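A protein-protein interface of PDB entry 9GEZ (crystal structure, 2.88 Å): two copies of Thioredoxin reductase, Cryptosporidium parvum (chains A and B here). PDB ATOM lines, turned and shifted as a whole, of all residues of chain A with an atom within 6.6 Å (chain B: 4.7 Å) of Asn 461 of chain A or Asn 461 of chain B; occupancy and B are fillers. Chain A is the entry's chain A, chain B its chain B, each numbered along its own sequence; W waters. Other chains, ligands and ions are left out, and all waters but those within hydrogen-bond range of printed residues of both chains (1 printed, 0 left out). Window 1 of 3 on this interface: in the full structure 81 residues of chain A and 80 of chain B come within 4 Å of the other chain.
N of Asp 492 of chain A lies within hydrogen-bond range of OE2 of Glu 464 of chain B (2.8 Å).
The side-chain carboxylate (OE1) of Glu 382 of chain A sits at hydrogen-bond distance from the backbone NH (N) of Asn 461 of chain A (3.4 Å). OE1 of Glu 382 of chain B lies within hydrogen-bond range of N of Asn 461 of chain B (3.3 Å).
Among the printed residues, merely in contact across the chains: Asn 461 of chain A with Asn 461 of chain B (3.5 Å), Ile 465 of chain A with Glu 464 of chain B (3.5 Å), Glu 464 of chain A with Ile 465 of chain B (3.6 Å) and Glu 464 of chain A with Glu 464 of chain B (3.9 Å).
Asn 461 of chain A touches just one residue of chain B: Asn 461. Asn 461 of chain B touches just one residue of chain A: Asn 461. Printed residues of chain B within 4 Å of Glu 464 of chain A: Glu 464 (3.9 Å) and Ile 465 (3.6 Å). Of the printed residues of chain B, Ile 465 of chain A touches Glu 464. Of the printed residues of chain A, Glu 464 of chain B touches Glu 464 (3.9 Å), Ile 465 (3.5 Å) and Asp 492 (2.8 Å). The nearest printed residue of chain B that does not touch Asn 461 of chain A is Glu 464 of chain B (4.8 Å). The nearest residue of chain A that does not touch Asn 461 of chain B is Glu 464 of chain A (4.4 Å). The nearest printed residue of chain B that does not touch Asp 492 of chain A is Gly 463 of chain B (6.9 Å).
Of the 8 printed residues of chain B, 3 touch a printed residue of chain A. Hydrophobic or aromatic side chains of chain B that line the printed part of chain A: Ile 465. Printed residues of chain A that touch a printed residue of chain B: Asn 461, Glu 464, Ile 465 and Asp 492. Hydrophobic or aromatic side chains of chain A within 4 Å of the printed part of chain B: Ile 465. Among the printed residues, 5 pairs touch across the chains. Among the printed residues, no Asp or Glu carboxylate lies within 4 Å of a Lys or Arg side-chain nitrogen of the other chain.
Asn 461 of chain B touches its own counterpart, Asn 461 of chain A. Glu 464 of chain B touches its own counterpart, Glu 464 of chain A. Glu 464 of chain A touches Ile 465 of chain B, and with the chains exchanged Ile 465 of chain A touches Glu 464 of chain B. Positions printed for both chains: 382, 459, 460, 461, 462, 463, 464 and 465. Of the 5 pairs that touch across the chains among the printed residues, 4 have their exchanged pair printed and touching as well.
Water W1 bridges the backbone carbonyl oxygen of Glu 464 of chain A and the backbone carbonyl oxygen of Ile 465 of chain B.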
ATOM      1  N   LEU A  90      -4.887 -10.993   9.196  1.00  0.00           N
ATOM      2  CA  LEU A  90      -5.031 -10.817   7.724  1.00  0.00           C
ATOM      3  C   LEU A  90      -6.515 -10.967   7.383  1.00  0.00           C
ATOM      4  O   LEU A  90      -7.025 -10.080   6.671  1.00  0.00           O
ATOM      5  CB  LEU A  90      -4.175 -11.834   6.963  1.00  0.00           C
ATOM      6  CG  LEU A  90      -2.679 -11.526   6.830  1.00  0.00           C
ATOM      7  CD1 LEU A  90      -2.037 -12.392   5.768  1.00  0.00           C
ATOM      8  CD2 LEU A  90      -2.404 -10.057   6.526  1.00  0.00           C
ATOM      9  N   THR A 376      11.438 -13.975   6.633  1.00  0.00           N
ATOM     10  CA  THR A 376      10.280 -13.055   6.433  1.00  0.00           C
ATOM     11  C   THR A 376       9.699 -12.676   7.791  1.00  0.00           C
ATOM     12  O   THR A 376       9.402 -13.577   8.565  1.00  0.00           O
ATOM     13  CB  THR A 376       9.165 -13.655   5.577  1.00  0.00           C
ATOM     14  OG1 THR A 376       9.680 -13.814   4.271  1.00  0.00           O
ATOM     15  CG2 THR A 376       7.958 -12.755   5.469  1.00  0.00           C
ATOM     16  N   PHE A 378       6.383 -11.346   9.502  1.00  0.00           N
ATOM     17  CA  PHE A 378       4.935 -11.326   9.206  1.00  0.00           C
ATOM     18  C   PHE A 378       4.302 -10.168   9.987  1.00  0.00           C
ATOM     19  O   PHE A 378       3.253 -10.387  10.640  1.00  0.00           O
ATOM     20  CB  PHE A 378       4.286 -12.690   9.472  1.00  0.00           C
ATOM     21  CG  PHE A 378       4.837 -13.792   8.602  1.00  0.00           C
ATOM     22  CD1 PHE A 378       5.963 -14.496   8.997  1.00  0.00           C
ATOM     23  CD2 PHE A 378       4.291 -14.062   7.357  1.00  0.00           C
ATOM     24  CE1 PHE A 378       6.498 -15.489   8.189  1.00  0.00           C
ATOM     25  CE2 PHE A 378       4.851 -15.032   6.542  1.00  0.00           C
ATOM     26  CZ  PHE A 378       5.940 -15.760   6.965  1.00  0.00           C
ATOM     27  N   GLU A 382       4.051  -7.950   5.273  1.00  0.00           N
ATOM     28  CA  GLU A 382       5.144  -8.927   5.451  1.00  0.00           C
ATOM     29  C   GLU A 382       6.364  -8.371   4.725  1.00  0.00           C
ATOM     30  O   GLU A 382       6.188  -7.787   3.629  1.00  0.00           O
ATOM     31  CB  GLU A 382       4.716 -10.293   4.892  1.00  0.00           C
ATOM     32  CG  GLU A 382       3.325 -10.695   5.309  1.00  0.00           C
ATOM     33  CD  GLU A 382       2.967 -12.140   5.012  1.00  0.00           C
ATOM     34  OE1 GLU A 382       3.740 -12.884   4.314  1.00  0.00           O
ATOM     35  OE2 GLU A 382       1.912 -12.553   5.525  1.00  0.00           O
ATOM     36  N   PHE A 457      11.561  -7.359  -0.327  1.00  0.00           N
ATOM     37  CA  PHE A 457      10.152  -7.157  -0.733  1.00  0.00           C
ATOM     38  C   PHE A 457       9.305  -6.903   0.496  1.00  0.00           C
ATOM     39  O   PHE A 457       9.329  -7.776   1.363  1.00  0.00           O
ATOM     40  CB  PHE A 457       9.605  -8.334  -1.545  1.00  0.00           C
ATOM     41  CG  PHE A 457       8.173  -8.126  -1.955  1.00  0.00           C
ATOM     42  CD1 PHE A 457       7.846  -7.242  -2.976  1.00  0.00           C
ATOM     43  CD2 PHE A 457       7.159  -8.767  -1.273  1.00  0.00           C
ATOM     44  CE1 PHE A 457       6.525  -6.997  -3.310  1.00  0.00           C
ATOM     45  CE2 PHE A 457       5.842  -8.569  -1.642  1.00  0.00           C
ATOM     46  CZ  PHE A 457       5.531  -7.677  -2.651  1.00  0.00           C
ATOM     47  N   GLY A 459       5.448  -6.540   1.455  1.00  0.00           N
ATOM     48  CA  GLY A 459       4.078  -6.740   0.948  1.00  0.00           C
ATOM     49  C   GLY A 459       3.389  -7.968   1.538  1.00  0.00           C
ATOM     50  O   GLY A 459       3.831  -8.530   2.546  1.00  0.00           O
ATOM     51  N   PRO A 460       2.253  -8.388   0.925  1.00  0.00           N
ATOM     52  CA  PRO A 460       1.534  -9.584   1.329  1.00  0.00           C
ATOM     53  C   PRO A 460       2.371 -10.721   0.771  1.00  0.00           C
ATOM     54  O   PRO A 460       3.087 -10.416  -0.157  1.00  0.00           O
ATOM     55  CB  PRO A 460       0.159  -9.475   0.688  1.00  0.00           C
ATOM     56  CG  PRO A 460       0.128  -8.110   0.055  1.00  0.00           C
ATOM     57  CD  PRO A 460       1.571  -7.711  -0.175  1.00  0.00           C
ATOM     58  N   ASN A 461       2.345 -11.906   1.398  1.00  0.00           N
ATOM     59  CA  ASN A 461       3.009 -13.107   0.846  1.00  0.00           C
ATOM     60  C   ASN A 461       4.472 -12.786   0.474  1.00  0.00           C
ATOM     61  O   ASN A 461       4.982 -13.349  -0.523  1.00  0.00           O
ATOM     62  CB  ASN A 461       2.203 -13.596  -0.356  1.00  0.00           C
ATOM     63  CG  ASN A 461       0.704 -13.583  -0.080  1.00  0.00           C
ATOM     64  OD1 ASN A 461       0.212 -14.278   0.817  1.00  0.00           O
ATOM     65  ND2 ASN A 461      -0.047 -12.841  -0.874  1.00  0.00           N
ATOM     66  N   ALA A 462       5.175 -11.945   1.237  1.00  0.00           N
ATOM     67  CA  ALA A 462       6.602 -11.640   0.993  1.00  0.00           C
ATOM     68  C   ALA A 462       7.451 -12.904   0.975  1.00  0.00           C
ATOM     69  O   ALA A 462       8.192 -13.063   0.009  1.00  0.00           O
ATOM     70  CB  ALA A 462       7.147 -10.733   2.044  1.00  0.00           C
ATOM     71  N   GLY A 463       7.419 -13.714   2.038  1.00  0.00           N
ATOM     72  CA  GLY A 463       8.058 -15.052   2.033  1.00  0.00           C
ATOM     73  C   GLY A 463       7.690 -15.904   0.808  1.00  0.00           C
ATOM     74  O   GLY A 463       8.645 -16.400   0.142  1.00  0.00           O
ATOM     75  N   GLU A 464       6.391 -16.110   0.518  1.00  0.00           N
ATOM     76  CA  GLU A 464       5.994 -16.921  -0.680  1.00  0.00           C
ATOM     77  C   GLU A 464       6.742 -16.333  -1.879  1.00  0.00           C
ATOM     78  O   GLU A 464       7.310 -17.120  -2.640  1.00  0.00           O
ATOM     79  CB  GLU A 464       4.479 -16.964  -0.969  1.00  0.00           C
ATOM     80  CG  GLU A 464       3.605 -17.598   0.136  1.00  0.00           C
ATOM     81  CD  GLU A 464       4.022 -18.908   0.824  1.00  0.00           C
ATOM     82  OE1 GLU A 464       4.557 -19.829   0.173  1.00  0.00           O
ATOM     83  OE2 GLU A 464       3.765 -19.039   2.010  1.00  0.00           O
ATOM     84  N   ILE A 465       6.844 -14.998  -1.965  1.00  0.00           N
ATOM     85  CA  ILE A 465       7.601 -14.291  -3.045  1.00  0.00           C
ATOM     86  C   ILE A 465       9.130 -14.389  -2.864  1.00  0.00           C
ATOM     87  O   ILE A 465       9.859 -14.517  -3.876  1.00  0.00           O
ATOM     88  CB  ILE A 465       7.151 -12.827  -3.098  1.00  0.00           C
ATOM     89  CG1 ILE A 465       5.663 -12.692  -3.420  1.00  0.00           C
ATOM     90  CG2 ILE A 465       7.991 -12.059  -4.099  1.00  0.00           C
ATOM     91  CD1 ILE A 465       5.153 -11.301  -3.166  1.00  0.00           C
ATOM     92  N   THR A 466       9.640 -14.216  -1.650  1.00  0.00           N
ATOM     93  CA  THR A 466      11.091 -14.198  -1.338  1.00  0.00           C
ATOM     94  C   THR A 466      11.740 -15.525  -1.731  1.00  0.00           C
ATOM     95  O   THR A 466      12.952 -15.487  -2.071  1.00  0.00           O
ATOM     96  CB  THR A 466      11.363 -14.077   0.160  1.00  0.00           C
ATOM     97  OG1 THR A 466      10.678 -12.971   0.748  1.00  0.00           O
ATOM     98  CG2 THR A 466      12.844 -13.989   0.439  1.00  0.00           C
ATOM     99  N   ASP A 492       2.327  -9.556  -7.646  1.00  0.00           N
ATOM    100  CA  ASP A 492       3.286  -8.553  -7.139  1.00  0.00           C
ATOM    101  C   ASP A 492       4.701  -9.022  -7.496  1.00  0.00           C
ATOM    102  O   ASP A 492       5.575  -8.167  -7.710  1.00  0.00           O
ATOM    103  CB  ASP A 492       2.997  -8.265  -5.666  1.00  0.00           C
ATOM    104  CG  ASP A 492       1.584  -7.720  -5.513  1.00  0.00           C
ATOM    105  OD1 ASP A 492       1.245  -6.790  -6.279  1.00  0.00           O
ATOM    106  OD2 ASP A 492       0.807  -8.280  -4.727  1.00  0.00           O
ATOM    107  N   GLU B 382      -4.962 -22.054  -7.041  1.00  0.00           N
ATOM    108  CA  GLU B 382      -4.187 -21.475  -8.167  1.00  0.00           C
ATOM    109  C   GLU B 382      -3.088 -22.479  -8.537  1.00  0.00           C
ATOM    110  O   GLU B 382      -2.537 -23.129  -7.608  1.00  0.00           O
ATOM    111  CB  GLU B 382      -3.605 -20.114  -7.767  1.00  0.00           C
ATOM    112  CG  GLU B 382      -4.594 -19.256  -6.978  1.00  0.00           C
ATOM    113  CD  GLU B 382      -3.945 -18.063  -6.336  1.00  0.00           C
ATOM    114  OE1 GLU B 382      -2.783 -17.773  -6.729  1.00  0.00           O
ATOM    115  OE2 GLU B 382      -4.581 -17.449  -5.450  1.00  0.00           O
ATOM    116  N   GLY B 459      -1.647 -24.284  -5.495  1.00  0.00           N
ATOM    117  CA  GLY B 459      -2.113 -23.817  -4.178  1.00  0.00           C
ATOM    118  C   GLY B 459      -2.521 -22.352  -4.193  1.00  0.00           C
ATOM    119  O   GLY B 459      -2.816 -21.781  -5.252  1.00  0.00           O
ATOM    120  N   PRO B 460      -2.546 -21.730  -3.000  1.00  0.00           N
ATOM    121  CA  PRO B 460      -2.850 -20.324  -2.853  1.00  0.00           C
ATOM    122  C   PRO B 460      -1.562 -19.651  -3.290  1.00  0.00           C
ATOM    123  O   PRO B 460      -0.521 -20.349  -3.239  1.00  0.00           O
ATOM    124  CB  PRO B 460      -3.100 -20.117  -1.364  1.00  0.00           C
ATOM    125  CG  PRO B 460      -3.120 -21.506  -0.780  1.00  0.00           C
ATOM    126  CD  PRO B 460      -2.261 -22.349  -1.709  1.00  0.00           C
ATOM    127  N   ASN B 461      -1.642 -18.394  -3.739  1.00  0.00           N
ATOM    128  CA  ASN B 461      -0.443 -17.581  -4.032  1.00  0.00           C
ATOM    129  C   ASN B 461       0.541 -18.396  -4.889  1.00  0.00           C
ATOM    130  O   ASN B 461       1.793 -18.262  -4.689  1.00  0.00           O
ATOM    131  CB  ASN B 461       0.205 -17.143  -2.723  1.00  0.00           C
ATOM    132  CG  ASN B 461      -0.797 -16.773  -1.651  1.00  0.00           C
ATOM    133  OD1 ASN B 461      -1.575 -15.846  -1.832  1.00  0.00           O
ATOM    134  ND2 ASN B 461      -0.766 -17.469  -0.533  1.00  0.00           N
ATOM    135  N   ALA B 462       0.015 -19.205  -5.813  1.00  0.00           N
ATOM    136  CA  ALA B 462       0.775 -19.723  -6.970  1.00  0.00           C
ATOM    137  C   ALA B 462       0.819 -18.556  -7.958  1.00  0.00           C
ATOM    138  O   ALA B 462      -0.172 -17.792  -7.982  1.00  0.00           O
ATOM    139  CB  ALA B 462       0.123 -20.942  -7.583  1.00  0.00           C
ATOM    140  N   GLY B 463       1.911 -18.404  -8.697  1.00  0.00           N
ATOM    141  CA  GLY B 463       2.261 -17.130  -9.368  1.00  0.00           C
ATOM    142  C   GLY B 463       3.172 -16.310  -8.466  1.00  0.00           C
ATOM    143  O   GLY B 463       4.413 -16.272  -8.736  1.00  0.00           O
ATOM    144  N   GLU B 464       2.637 -15.831  -7.340  1.00  0.00           N
ATOM    145  CA  GLU B 464       3.476 -15.243  -6.259  1.00  0.00           C
ATOM    146  C   GLU B 464       4.627 -16.206  -5.958  1.00  0.00           C
ATOM    147  O   GLU B 464       5.748 -15.743  -5.913  1.00  0.00           O
ATOM    148  CB  GLU B 464       2.650 -14.904  -5.015  1.00  0.00           C
ATOM    149  CG  GLU B 464       1.574 -13.855  -5.267  1.00  0.00           C
ATOM    150  CD  GLU B 464       2.140 -12.559  -5.823  1.00  0.00           C
ATOM    151  OE1 GLU B 464       3.361 -12.522  -6.086  1.00  0.00           O
ATOM    152  OE2 GLU B 464       1.362 -11.596  -5.988  1.00  0.00           O
ATOM    153  N   ILE B 465       4.357 -17.509  -5.814  1.00  0.00           N
ATOM    154  CA  ILE B 465       5.418 -18.546  -5.609  1.00  0.00           C
ATOM    155  C   ILE B 465       6.175 -18.837  -6.931  1.00  0.00           C
ATOM    156  O   ILE B 465       7.415 -19.035  -6.887  1.00  0.00           O
ATOM    157  CB  ILE B 465       4.784 -19.829  -5.046  1.00  0.00           C
ATOM    158  CG1 ILE B 465       4.251 -19.613  -3.648  1.00  0.00           C
ATOM    159  CG2 ILE B 465       5.772 -20.979  -5.055  1.00  0.00           C
ATOM    160  CD1 ILE B 465       3.500 -20.789  -3.112  1.00  0.00           C
HETATM  161  O   HOH W   1       8.526 -18.551  -4.395  1.00  0.00           O
